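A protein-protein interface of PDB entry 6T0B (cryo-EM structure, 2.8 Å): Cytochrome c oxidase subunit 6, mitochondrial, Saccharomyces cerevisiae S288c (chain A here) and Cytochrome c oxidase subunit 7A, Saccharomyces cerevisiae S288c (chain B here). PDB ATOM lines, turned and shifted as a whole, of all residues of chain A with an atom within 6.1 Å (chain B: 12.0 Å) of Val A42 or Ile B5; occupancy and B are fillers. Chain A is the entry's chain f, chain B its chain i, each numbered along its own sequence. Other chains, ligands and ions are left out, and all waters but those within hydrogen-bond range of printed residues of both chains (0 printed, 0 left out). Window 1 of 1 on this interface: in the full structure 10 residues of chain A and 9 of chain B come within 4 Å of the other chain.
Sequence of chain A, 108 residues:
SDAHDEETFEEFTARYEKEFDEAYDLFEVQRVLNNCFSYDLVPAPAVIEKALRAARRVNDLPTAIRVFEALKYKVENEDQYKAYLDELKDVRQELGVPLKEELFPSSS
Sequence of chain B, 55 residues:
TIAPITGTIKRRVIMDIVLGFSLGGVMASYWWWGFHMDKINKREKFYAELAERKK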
ATOM      1  N   PHE A   9      17.328  30.814  12.231  1.00  0.00           N
ATOM      2  CA  PHE A   9      17.924  29.718  12.975  1.00  0.00           C
ATOM      3  C   PHE A   9      18.629  28.736  12.048  1.00  0.00           C
ATOM      4  O   PHE A   9      19.682  28.188  12.400  1.00  0.00           O
ATOM      5  CB  PHE A   9      16.842  29.026  13.787  1.00  0.00           C
ATOM      6  CG  PHE A   9      17.369  28.126  14.834  1.00  0.00           C
ATOM      7  CD1 PHE A   9      17.897  28.639  15.993  1.00  0.00           C
ATOM      8  CD2 PHE A   9      17.335  26.763  14.662  1.00  0.00           C
ATOM      9  CE1 PHE A   9      18.394  27.805  16.963  1.00  0.00           C
ATOM     10  CE2 PHE A   9      17.822  25.924  15.625  1.00  0.00           C
ATOM     11  CZ  PHE A   9      18.357  26.445  16.776  1.00  0.00           C
ATOM     12  N   PHE A  37      28.172  29.140  21.495  1.00  0.00           N
ATOM     13  CA  PHE A  37      27.332  29.150  22.683  1.00  0.00           C
ATOM     14  C   PHE A  37      27.148  30.535  23.263  1.00  0.00           C
ATOM     15  O   PHE A  37      26.429  30.682  24.249  1.00  0.00           O
ATOM     16  CB  PHE A  37      27.901  28.238  23.750  1.00  0.00           C
ATOM     17  CG  PHE A  37      27.376  26.863  23.676  1.00  0.00           C
ATOM     18  CD1 PHE A  37      26.228  26.518  24.340  1.00  0.00           C
ATOM     19  CD2 PHE A  37      28.017  25.911  22.923  1.00  0.00           C
ATOM     20  CE1 PHE A  37      25.735  25.256  24.258  1.00  0.00           C
ATOM     21  CE2 PHE A  37      27.529  24.642  22.853  1.00  0.00           C
ATOM     22  CZ  PHE A  37      26.385  24.319  23.516  1.00  0.00           C
ATOM     23  N   TYR A  39      25.346  32.947  22.096  1.00  0.00           N
ATOM     24  CA  TYR A  39      24.219  33.529  21.391  1.00  0.00           C
ATOM     25  C   TYR A  39      22.973  33.247  22.198  1.00  0.00           C
ATOM     26  O   TYR A  39      22.995  32.462  23.144  1.00  0.00           O
ATOM     27  CB  TYR A  39      24.067  32.960  19.990  1.00  0.00           C
ATOM     28  CG  TYR A  39      24.942  33.597  18.958  1.00  0.00           C
ATOM     29  CD1 TYR A  39      26.194  33.102  18.691  1.00  0.00           C
ATOM     30  CD2 TYR A  39      24.504  34.679  18.237  1.00  0.00           C
ATOM     31  CE1 TYR A  39      26.984  33.677  17.749  1.00  0.00           C
ATOM     32  CE2 TYR A  39      25.291  35.254  17.294  1.00  0.00           C
ATOM     33  CZ  TYR A  39      26.534  34.746  17.056  1.00  0.00           C
ATOM     34  OH  TYR A  39      27.339  35.315  16.108  1.00  0.00           O
ATOM     35  N   ASP A  40      21.870  33.877  21.819  1.00  0.00           N
ATOM     36  CA  ASP A  40      20.611  33.673  22.531  1.00  0.00           C
ATOM     37  C   ASP A  40      19.762  32.616  21.827  1.00  0.00           C
ATOM     38  O   ASP A  40      18.698  32.880  21.284  1.00  0.00           O
ATOM     39  CB  ASP A  40      19.864  34.987  22.678  1.00  0.00           C
ATOM     40  CG  ASP A  40      18.727  34.883  23.648  1.00  0.00           C
ATOM     41  OD1 ASP A  40      18.757  33.956  24.477  1.00  0.00           O
ATOM     42  OD2 ASP A  40      17.793  35.701  23.571  1.00  0.00           O
ATOM     43  N   LEU A  41      20.264  31.393  21.890  1.00  0.00           N
ATOM     44  CA  LEU A  41      19.645  30.198  21.351  1.00  0.00           C
ATOM     45  C   LEU A  41      20.448  29.024  21.858  1.00  0.00           C
ATOM     46  O   LEU A  41      21.667  29.123  21.971  1.00  0.00           O
ATOM     47  CB  LEU A  41      19.631  30.212  19.821  1.00  0.00           C
ATOM     48  CG  LEU A  41      20.928  30.427  19.060  1.00  0.00           C
ATOM     49  CD1 LEU A  41      21.493  29.109  18.586  1.00  0.00           C
ATOM     50  CD2 LEU A  41      20.678  31.340  17.906  1.00  0.00           C
ATOM     51  N   VAL A  42      19.786  27.922  22.177  1.00  0.00           N
ATOM     52  CA  VAL A  42      20.599  26.737  22.377  1.00  0.00           C
ATOM     53  C   VAL A  42      20.867  26.282  20.954  1.00  0.00           C
ATOM     54  O   VAL A  42      20.005  26.460  20.081  1.00  0.00           O
ATOM     55  CB  VAL A  42      19.945  25.677  23.278  1.00  0.00           C
ATOM     56  CG1 VAL A  42      18.797  24.971  22.607  1.00  0.00           C
ATOM     57  CG2 VAL A  42      20.987  24.680  23.751  1.00  0.00           C
ATOM     58  N   PRO A  43      22.085  25.856  20.644  1.00  0.00           N
ATOM     59  CA  PRO A  43      22.358  25.313  19.320  1.00  0.00           C
ATOM     60  C   PRO A  43      21.513  24.084  19.036  1.00  0.00           C
ATOM     61  O   PRO A  43      21.089  23.369  19.942  1.00  0.00           O
ATOM     62  CB  PRO A  43      23.839  24.964  19.401  1.00  0.00           C
ATOM     63  CG  PRO A  43      24.372  25.913  20.324  1.00  0.00           C
ATOM     64  CD  PRO A  43      23.334  26.175  21.346  1.00  0.00           C
ATOM     65  N   ALA A  44      21.258  23.856  17.759  1.00  0.00           N
ATOM     66  CA  ALA A  44      20.539  22.684  17.309  1.00  0.00           C
ATOM     67  C   ALA A  44      21.350  21.420  17.597  1.00  0.00           C
ATOM     68  O   ALA A  44      22.547  21.496  17.868  1.00  0.00           O
ATOM     69  CB  ALA A  44      20.250  22.822  15.817  1.00  0.00           C
ATOM     70  N   LEU A  71      25.695  22.927  27.213  1.00  0.00           N
ATOM     71  CA  LEU A  71      24.283  22.915  26.857  1.00  0.00           C
ATOM     72  C   LEU A  71      23.395  22.617  28.047  1.00  0.00           C
ATOM     73  O   LEU A  71      22.212  22.958  28.008  1.00  0.00           O
ATOM     74  CB  LEU A  71      23.987  21.956  25.706  1.00  0.00           C
ATOM     75  CG  LEU A  71      24.205  20.459  25.712  1.00  0.00           C
ATOM     76  CD1 LEU A  71      22.976  19.723  26.160  1.00  0.00           C
ATOM     77  CD2 LEU A  71      24.548  20.046  24.311  1.00  0.00           C
ATOM     78  N   LYS A  74      22.902  25.935  29.110  1.00  0.00           N
ATOM     79  CA  LYS A  74      22.286  26.728  28.060  1.00  0.00           C
ATOM     80  C   LYS A  74      20.795  26.470  27.897  1.00  0.00           C
ATOM     81  O   LYS A  74      20.056  27.394  27.551  1.00  0.00           O
ATOM     82  CB  LYS A  74      23.004  26.466  26.742  1.00  0.00           C
ATOM     83  CG  LYS A  74      22.890  27.578  25.741  1.00  0.00           C
ATOM     84  CD  LYS A  74      23.518  28.832  26.252  1.00  0.00           C
ATOM     85  CE  LYS A  74      23.213  29.989  25.354  1.00  0.00           C
ATOM     86  NZ  LYS A  74      23.493  31.235  26.072  1.00  0.00           N
ATOM     87  N   VAL A  75      20.323  25.241  28.125  1.00  0.00           N
ATOM     88  CA  VAL A  75      18.899  24.984  27.949  1.00  0.00           C
ATOM     89  C   VAL A  75      18.110  25.564  29.112  1.00  0.00           C
ATOM     90  O   VAL A  75      18.645  25.887  30.172  1.00  0.00           O
ATOM     91  CB  VAL A  75      18.611  23.487  27.796  1.00  0.00           C
ATOM     92  CG1 VAL A  75      19.244  22.951  26.557  1.00  0.00           C
ATOM     93  CG2 VAL A  75      19.100  22.754  29.003  1.00  0.00           C
ATOM     94  N   GLU A  76      16.802  25.672  28.908  1.00  0.00           N
ATOM     95  CA  GLU A  76      15.924  26.262  29.910  1.00  0.00           C
ATOM     96  C   GLU A  76      15.491  25.272  30.983  1.00  0.00           C
ATOM     97  O   GLU A  76      15.322  25.664  32.141  1.00  0.00           O
ATOM     98  CB  GLU A  76      14.683  26.830  29.239  1.00  0.00           C
ATOM     99  CG  GLU A  76      14.925  27.979  28.310  1.00  0.00           C
ATOM    100  CD  GLU A  76      13.633  28.668  27.945  1.00  0.00           C
ATOM    101  OE1 GLU A  76      12.565  28.136  28.302  1.00  0.00           O
ATOM    102  OE2 GLU A  76      13.676  29.741  27.309  1.00  0.00           O
ATOM    103  N   GLN A  80      14.601  19.551  28.442  1.00  0.00           N
ATOM    104  CA  GLN A  80      15.278  19.872  27.191  1.00  0.00           C
ATOM    105  C   GLN A  80      16.666  19.257  27.154  1.00  0.00           C
ATOM    106  O   GLN A  80      17.113  18.773  26.110  1.00  0.00           O
ATOM    107  CB  GLN A  80      15.374  21.377  27.024  1.00  0.00           C
ATOM    108  CG  GLN A  80      14.074  22.071  27.156  1.00  0.00           C
ATOM    109  CD  GLN A  80      14.239  23.552  27.158  1.00  0.00           C
ATOM    110  OE1 GLN A  80      15.327  24.052  27.391  1.00  0.00           O
ATOM    111  NE2 GLN A  80      13.168  24.274  26.872  1.00  0.00           N
ATOM    112  N   TYR A  84      18.021  16.440  24.523  1.00  0.00           N
ATOM    113  CA  TYR A  84      19.308  16.440  23.835  1.00  0.00           C
ATOM    114  C   TYR A  84      20.056  15.148  24.104  1.00  0.00           C
ATOM    115  O   TYR A  84      20.661  14.563  23.200  1.00  0.00           O
ATOM    116  CB  TYR A  84      20.153  17.625  24.288  1.00  0.00           C
ATOM    117  CG  TYR A  84      19.989  18.840  23.432  1.00  0.00           C
ATOM    118  CD1 TYR A  84      18.908  19.680  23.600  1.00  0.00           C
ATOM    119  CD2 TYR A  84      20.903  19.142  22.442  1.00  0.00           C
ATOM    120  CE1 TYR A  84      18.746  20.788  22.814  1.00  0.00           C
ATOM    121  CE2 TYR A  84      20.744  20.253  21.655  1.00  0.00           C
ATOM    122  CZ  TYR A  84      19.662  21.061  21.851  1.00  0.00           C
ATOM    123  OH  TYR A  84      19.497  22.163  21.073  1.00  0.00           O
ATOM    124  N   THR B   1      11.401  15.254  17.070  1.00  0.00           N
ATOM    125  CA  THR B   1      12.349  16.330  16.819  1.00  0.00           C
ATOM    126  C   THR B   1      12.721  17.044  18.095  1.00  0.00           C
ATOM    127  O   THR B   1      12.169  16.765  19.155  1.00  0.00           O
ATOM    128  CB  THR B   1      11.783  17.373  15.860  1.00  0.00           C
ATOM    129  OG1 THR B   1      12.757  18.398  15.651  1.00  0.00           O
ATOM    130  CG2 THR B   1      10.543  18.003  16.453  1.00  0.00           C
ATOM    131  N   ILE B   2      13.663  17.968  17.991  1.00  0.00           N
ATOM    132  CA  ILE B   2      13.882  18.979  19.011  1.00  0.00           C
ATOM    133  C   ILE B   2      13.563  20.312  18.364  1.00  0.00           C
ATOM    134  O   ILE B   2      14.283  20.767  17.469  1.00  0.00           O
ATOM    135  CB  ILE B   2      15.308  18.963  19.564  1.00  0.00           C
ATOM    136  CG1 ILE B   2      15.629  17.597  20.166  1.00  0.00           C
ATOM    137  CG2 ILE B   2      15.460  20.048  20.603  1.00  0.00           C
ATOM    138  CD1 ILE B   2      16.892  17.563  20.986  1.00  0.00           C
ATOM    139  N   ALA B   3      12.471  20.924  18.795  1.00  0.00           N
ATOM    140  CA  ALA B   3      12.069  22.208  18.262  1.00  0.00           C
ATOM    141  C   ALA B   3      13.045  23.280  18.733  1.00  0.00           C
ATOM    142  O   ALA B   3      13.703  23.108  19.761  1.00  0.00           O
ATOM    143  CB  ALA B   3      10.651  22.537  18.714  1.00  0.00           C
ATOM    144  N   PRO B   4      13.195  24.366  17.977  1.00  0.00           N
ATOM    145  CA  PRO B   4      14.171  25.396  18.348  1.00  0.00           C
ATOM    146  C   PRO B   4      13.846  26.106  19.655  1.00  0.00           C
ATOM    147  O   PRO B   4      12.760  26.651  19.836  1.00  0.00           O
ATOM    148  CB  PRO B   4      14.118  26.354  17.163  1.00  0.00           C
ATOM    149  CG  PRO B   4      13.817  25.480  16.045  1.00  0.00           C
ATOM    150  CD  PRO B   4      12.826  24.488  16.560  1.00  0.00           C
ATOM    151  N   ILE B   5      14.811  26.083  20.564  1.00  0.00           N
ATOM    152  CA  ILE B   5      14.755  26.807  21.825  1.00  0.00           C
ATOM    153  C   ILE B   5      15.546  28.089  21.631  1.00  0.00           C
ATOM    154  O   ILE B   5      16.765  28.116  21.798  1.00  0.00           O
ATOM    155  CB  ILE B   5      15.328  25.985  22.973  1.00  0.00           C
ATOM    156  CG1 ILE B   5      14.740  24.587  22.968  1.00  0.00           C
ATOM    157  CG2 ILE B   5      15.105  26.680  24.290  1.00  0.00           C
ATOM    158  CD1 ILE B   5      15.504  23.632  23.824  1.00  0.00           C
ATOM    159  N   THR B   6      14.861  29.158  21.280  1.00  0.00           N
ATOM    160  CA  THR B   6      15.511  30.428  21.048  1.00  0.00           C
ATOM    161  C   THR B   6      14.831  31.497  21.879  1.00  0.00           C
ATOM    162  O   THR B   6      13.749  31.290  22.425  1.00  0.00           O
ATOM    163  CB  THR B   6      15.468  30.796  19.574  1.00  0.00           C
ATOM    164  OG1 THR B   6      16.152  32.037  19.369  1.00  0.00           O
ATOM    165  CG2 THR B   6      14.038  30.908  19.111  1.00  0.00           C
ATOM    166  N   GLY B   7      15.496  32.635  21.984  1.00  0.00           N
ATOM    167  CA  GLY B   7      14.948  33.799  22.638  1.00  0.00           C
ATOM    168  C   GLY B   7      14.590  33.651  24.097  1.00  0.00           C
ATOM    169  O   GLY B   7      13.419  33.781  24.442  1.00  0.00           O
ATOM    170  N   THR B   8      15.555  33.378  24.967  1.00  0.00           N
ATOM    171  CA  THR B   8      15.255  33.397  26.389  1.00  0.00           C
ATOM    172  C   THR B   8      15.680  34.691  27.043  1.00  0.00           C
ATOM    173  O   THR B   8      15.088  35.090  28.047  1.00  0.00           O
ATOM    174  CB  THR B   8      15.901  32.210  27.109  1.00  0.00           C
ATOM    175  OG1 THR B   8      15.530  32.235  28.489  1.00  0.00           O
ATOM    176  CG2 THR B   8      17.403  32.221  27.011  1.00  0.00           C
ATOM    177  N   ILE B   9      16.655  35.382  26.468  1.00  0.00           N
ATOM    178  CA  ILE B   9      17.036  36.674  26.994  1.00  0.00           C
ATOM    179  C   ILE B   9      16.015  37.705  26.587  1.00  0.00           C
ATOM    180  O   ILE B   9      15.770  38.653  27.329  1.00  0.00           O
ATOM    181  CB  ILE B   9      18.454  37.019  26.528  1.00  0.00           C
ATOM    182  CG1 ILE B   9      19.398  35.947  27.026  1.00  0.00           C
ATOM    183  CG2 ILE B   9      18.941  38.342  27.072  1.00  0.00           C
ATOM    184  CD1 ILE B   9      19.418  35.810  28.524  1.00  0.00           C
ATOM    185  N   LYS B  10      15.337  37.496  25.462  1.00  0.00           N
ATOM    186  CA  LYS B  10      14.288  38.408  25.036  1.00  0.00           C
ATOM    187  C   LYS B  10      13.126  38.402  26.016  1.00  0.00           C
ATOM    188  O   LYS B  10      12.777  39.442  26.591  1.00  0.00           O
ATOM    189  CB  LYS B  10      13.817  38.033  23.643  1.00  0.00           C
ATOM    190  CG  LYS B  10      13.499  39.217  22.775  1.00  0.00           C
ATOM    191  CD  LYS B  10      12.966  38.796  21.426  1.00  0.00           C
ATOM    192  CE  LYS B  10      11.606  38.139  21.556  1.00  0.00           C
ATOM    193  NZ  LYS B  10      11.136  37.619  20.249  1.00  0.00           N
ATOM    194  N   ARG B  11      12.553  37.228  26.272  1.00  0.00           N
ATOM    195  CA  ARG B  11      11.451  37.166  27.217  1.00  0.00           C
ATOM    196  C   ARG B  11      11.919  37.387  28.650  1.00  0.00           C
ATOM    197  O   ARG B  11      11.140  37.876  29.473  1.00  0.00           O
ATOM    198  CB  ARG B  11      10.689  35.849  27.052  1.00  0.00           C
ATOM    199  CG  ARG B  11      11.080  34.748  27.972  1.00  0.00           C
ATOM    200  CD  ARG B  11      10.243  33.539  27.711  1.00  0.00           C
ATOM    201  NE  ARG B  11      10.449  33.020  26.366  1.00  0.00           N
ATOM    202  CZ  ARG B  11      11.335  32.079  26.059  1.00  0.00           C
ATOM    203  NH1 ARG B  11      11.459  31.663  24.808  1.00  0.00           N
ATOM    204  NH2 ARG B  11      12.108  31.564  27.005  1.00  0.00           N
ATOM    205  N   ARG B  12      13.197  37.151  28.933  1.00  0.00           N
ATOM    206  CA  ARG B  12      13.725  37.415  30.262  1.00  0.00           C
ATOM    207  C   ARG B  12      13.833  38.909  30.539  1.00  0.00           C
ATOM    208  O   ARG B  12      13.436  39.370  31.611  1.00  0.00           O
ATOM    209  CB  ARG B  12      15.079  36.741  30.413  1.00  0.00           C
ATOM    210  CG  ARG B  12      15.620  36.761  31.793  1.00  0.00           C
ATOM    211  CD  ARG B  12      16.832  35.878  31.884  1.00  0.00           C
ATOM    212  NE  ARG B  12      16.478  34.474  31.973  1.00  0.00           N
ATOM    213  CZ  ARG B  12      17.339  33.513  32.273  1.00  0.00           C
ATOM    214  NH1 ARG B  12      18.604  33.810  32.507  1.00  0.00           N
ATOM    215  NH2 ARG B  12      16.937  32.255  32.339  1.00  0.00           N
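O of Asp A40 is in hydrogen-bond range of OG1 of Thr B6, at 3.3 Å.
N of Gly B7 is in hydrogen-bond range of O of Asp A40 (3.3 Å).
The side-chain carboxylate (OD1) of Asp A40 is in hydrogen-bond range of the backbone NH (N) of Thr B8 (3.3 Å).
OD2 of Asp A40 sits at hydrogen-bond distance from N of Ile B9 (3.1 Å).
The backbone carbonyl oxygen of Ile B5 sits at hydrogen-bond distance from the backbone NH of Val A42 (3.1 Å).
The side-chain carboxylate (OE2) of Glu A76 is in hydrogen-bond range of the side-chain hydroxyl (OG1) of Thr B8 (3.3 Å).
NH2 of Arg B11 is in salt-bridge range of OE2 of Glu A76, 2.4 Å away.
The side-chain amide oxygen (OE1) of Gln A80 sits at hydrogen-bond distance from the backbone NH (N) of Glu A76.
The guanidinium group (NH1) of Arg B11 sits at hydrogen-bond distance from the backbone carbonyl oxygen (O) of Thr B6 (3.3 Å).
O of Gly B7 is in hydrogen-bond range of NH1 of Arg B11 (2.9 Å).
Phe A9 touches Pro B4.
OD2 of Asp A40 touches N of Lys B10 (3.6 Å).
Leu A41 touches Ile B5 (CA to O, 3.6 Å).
Leu A41 touches Thr B6.
CD of Gln A80 touches CD1 of Ile B5, 3.6 Å away.
Ile B2 touches Tyr A84 (CD1 to N, 3.9 Å).
Val A42 touches just one residue of chain B: Ile B5 (3.1 Å).
Of chain A, only Leu A41, Val A42 and Gln A80 come within 4 Å of Ile B5.
No residue of chain B comes within 4 Å of Phe A37.
No residue of chain B comes within 4 Å of Pro A43.
No residue of chain B comes within 4 Å of Lys A74.
Glu A76 touches two residues of chain B.
Gln A80 touches just one residue of chain B: Ile B5 (3.6 Å).
Printed residues of chain A within 4 Å of Pro B4: Phe A9.
Printed residues of chain A within 4 Å of Lys B10: Asp A40 (3.6 Å).
Arg B12 touches none of the printed residues of chain A.
The nearest residue of chain A that does not touch Ile B5 is Glu A76 (4.2 Å).
The nearest printed residue of chain A that does not touch Ile B9 is Lys A74 (6.3 Å).
Of the 12 printed residues of chain B, 9 touch a printed residue of chain A.
Printed residues of chain B that touch a printed residue of chain A: Ile B2, Pro B4, Ile B5, Thr B6, Gly B7, Thr B8, Ile B9, Lys B10 and Arg B11.
Along chain B the printed residues that touch a printed residue of chain A span positions 2 to 11.
Hydrophobic or aromatic side chains of chain A within 4 Å of the printed part of chain B: Phe A9, Leu A41, Val A42 and Tyr A84.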
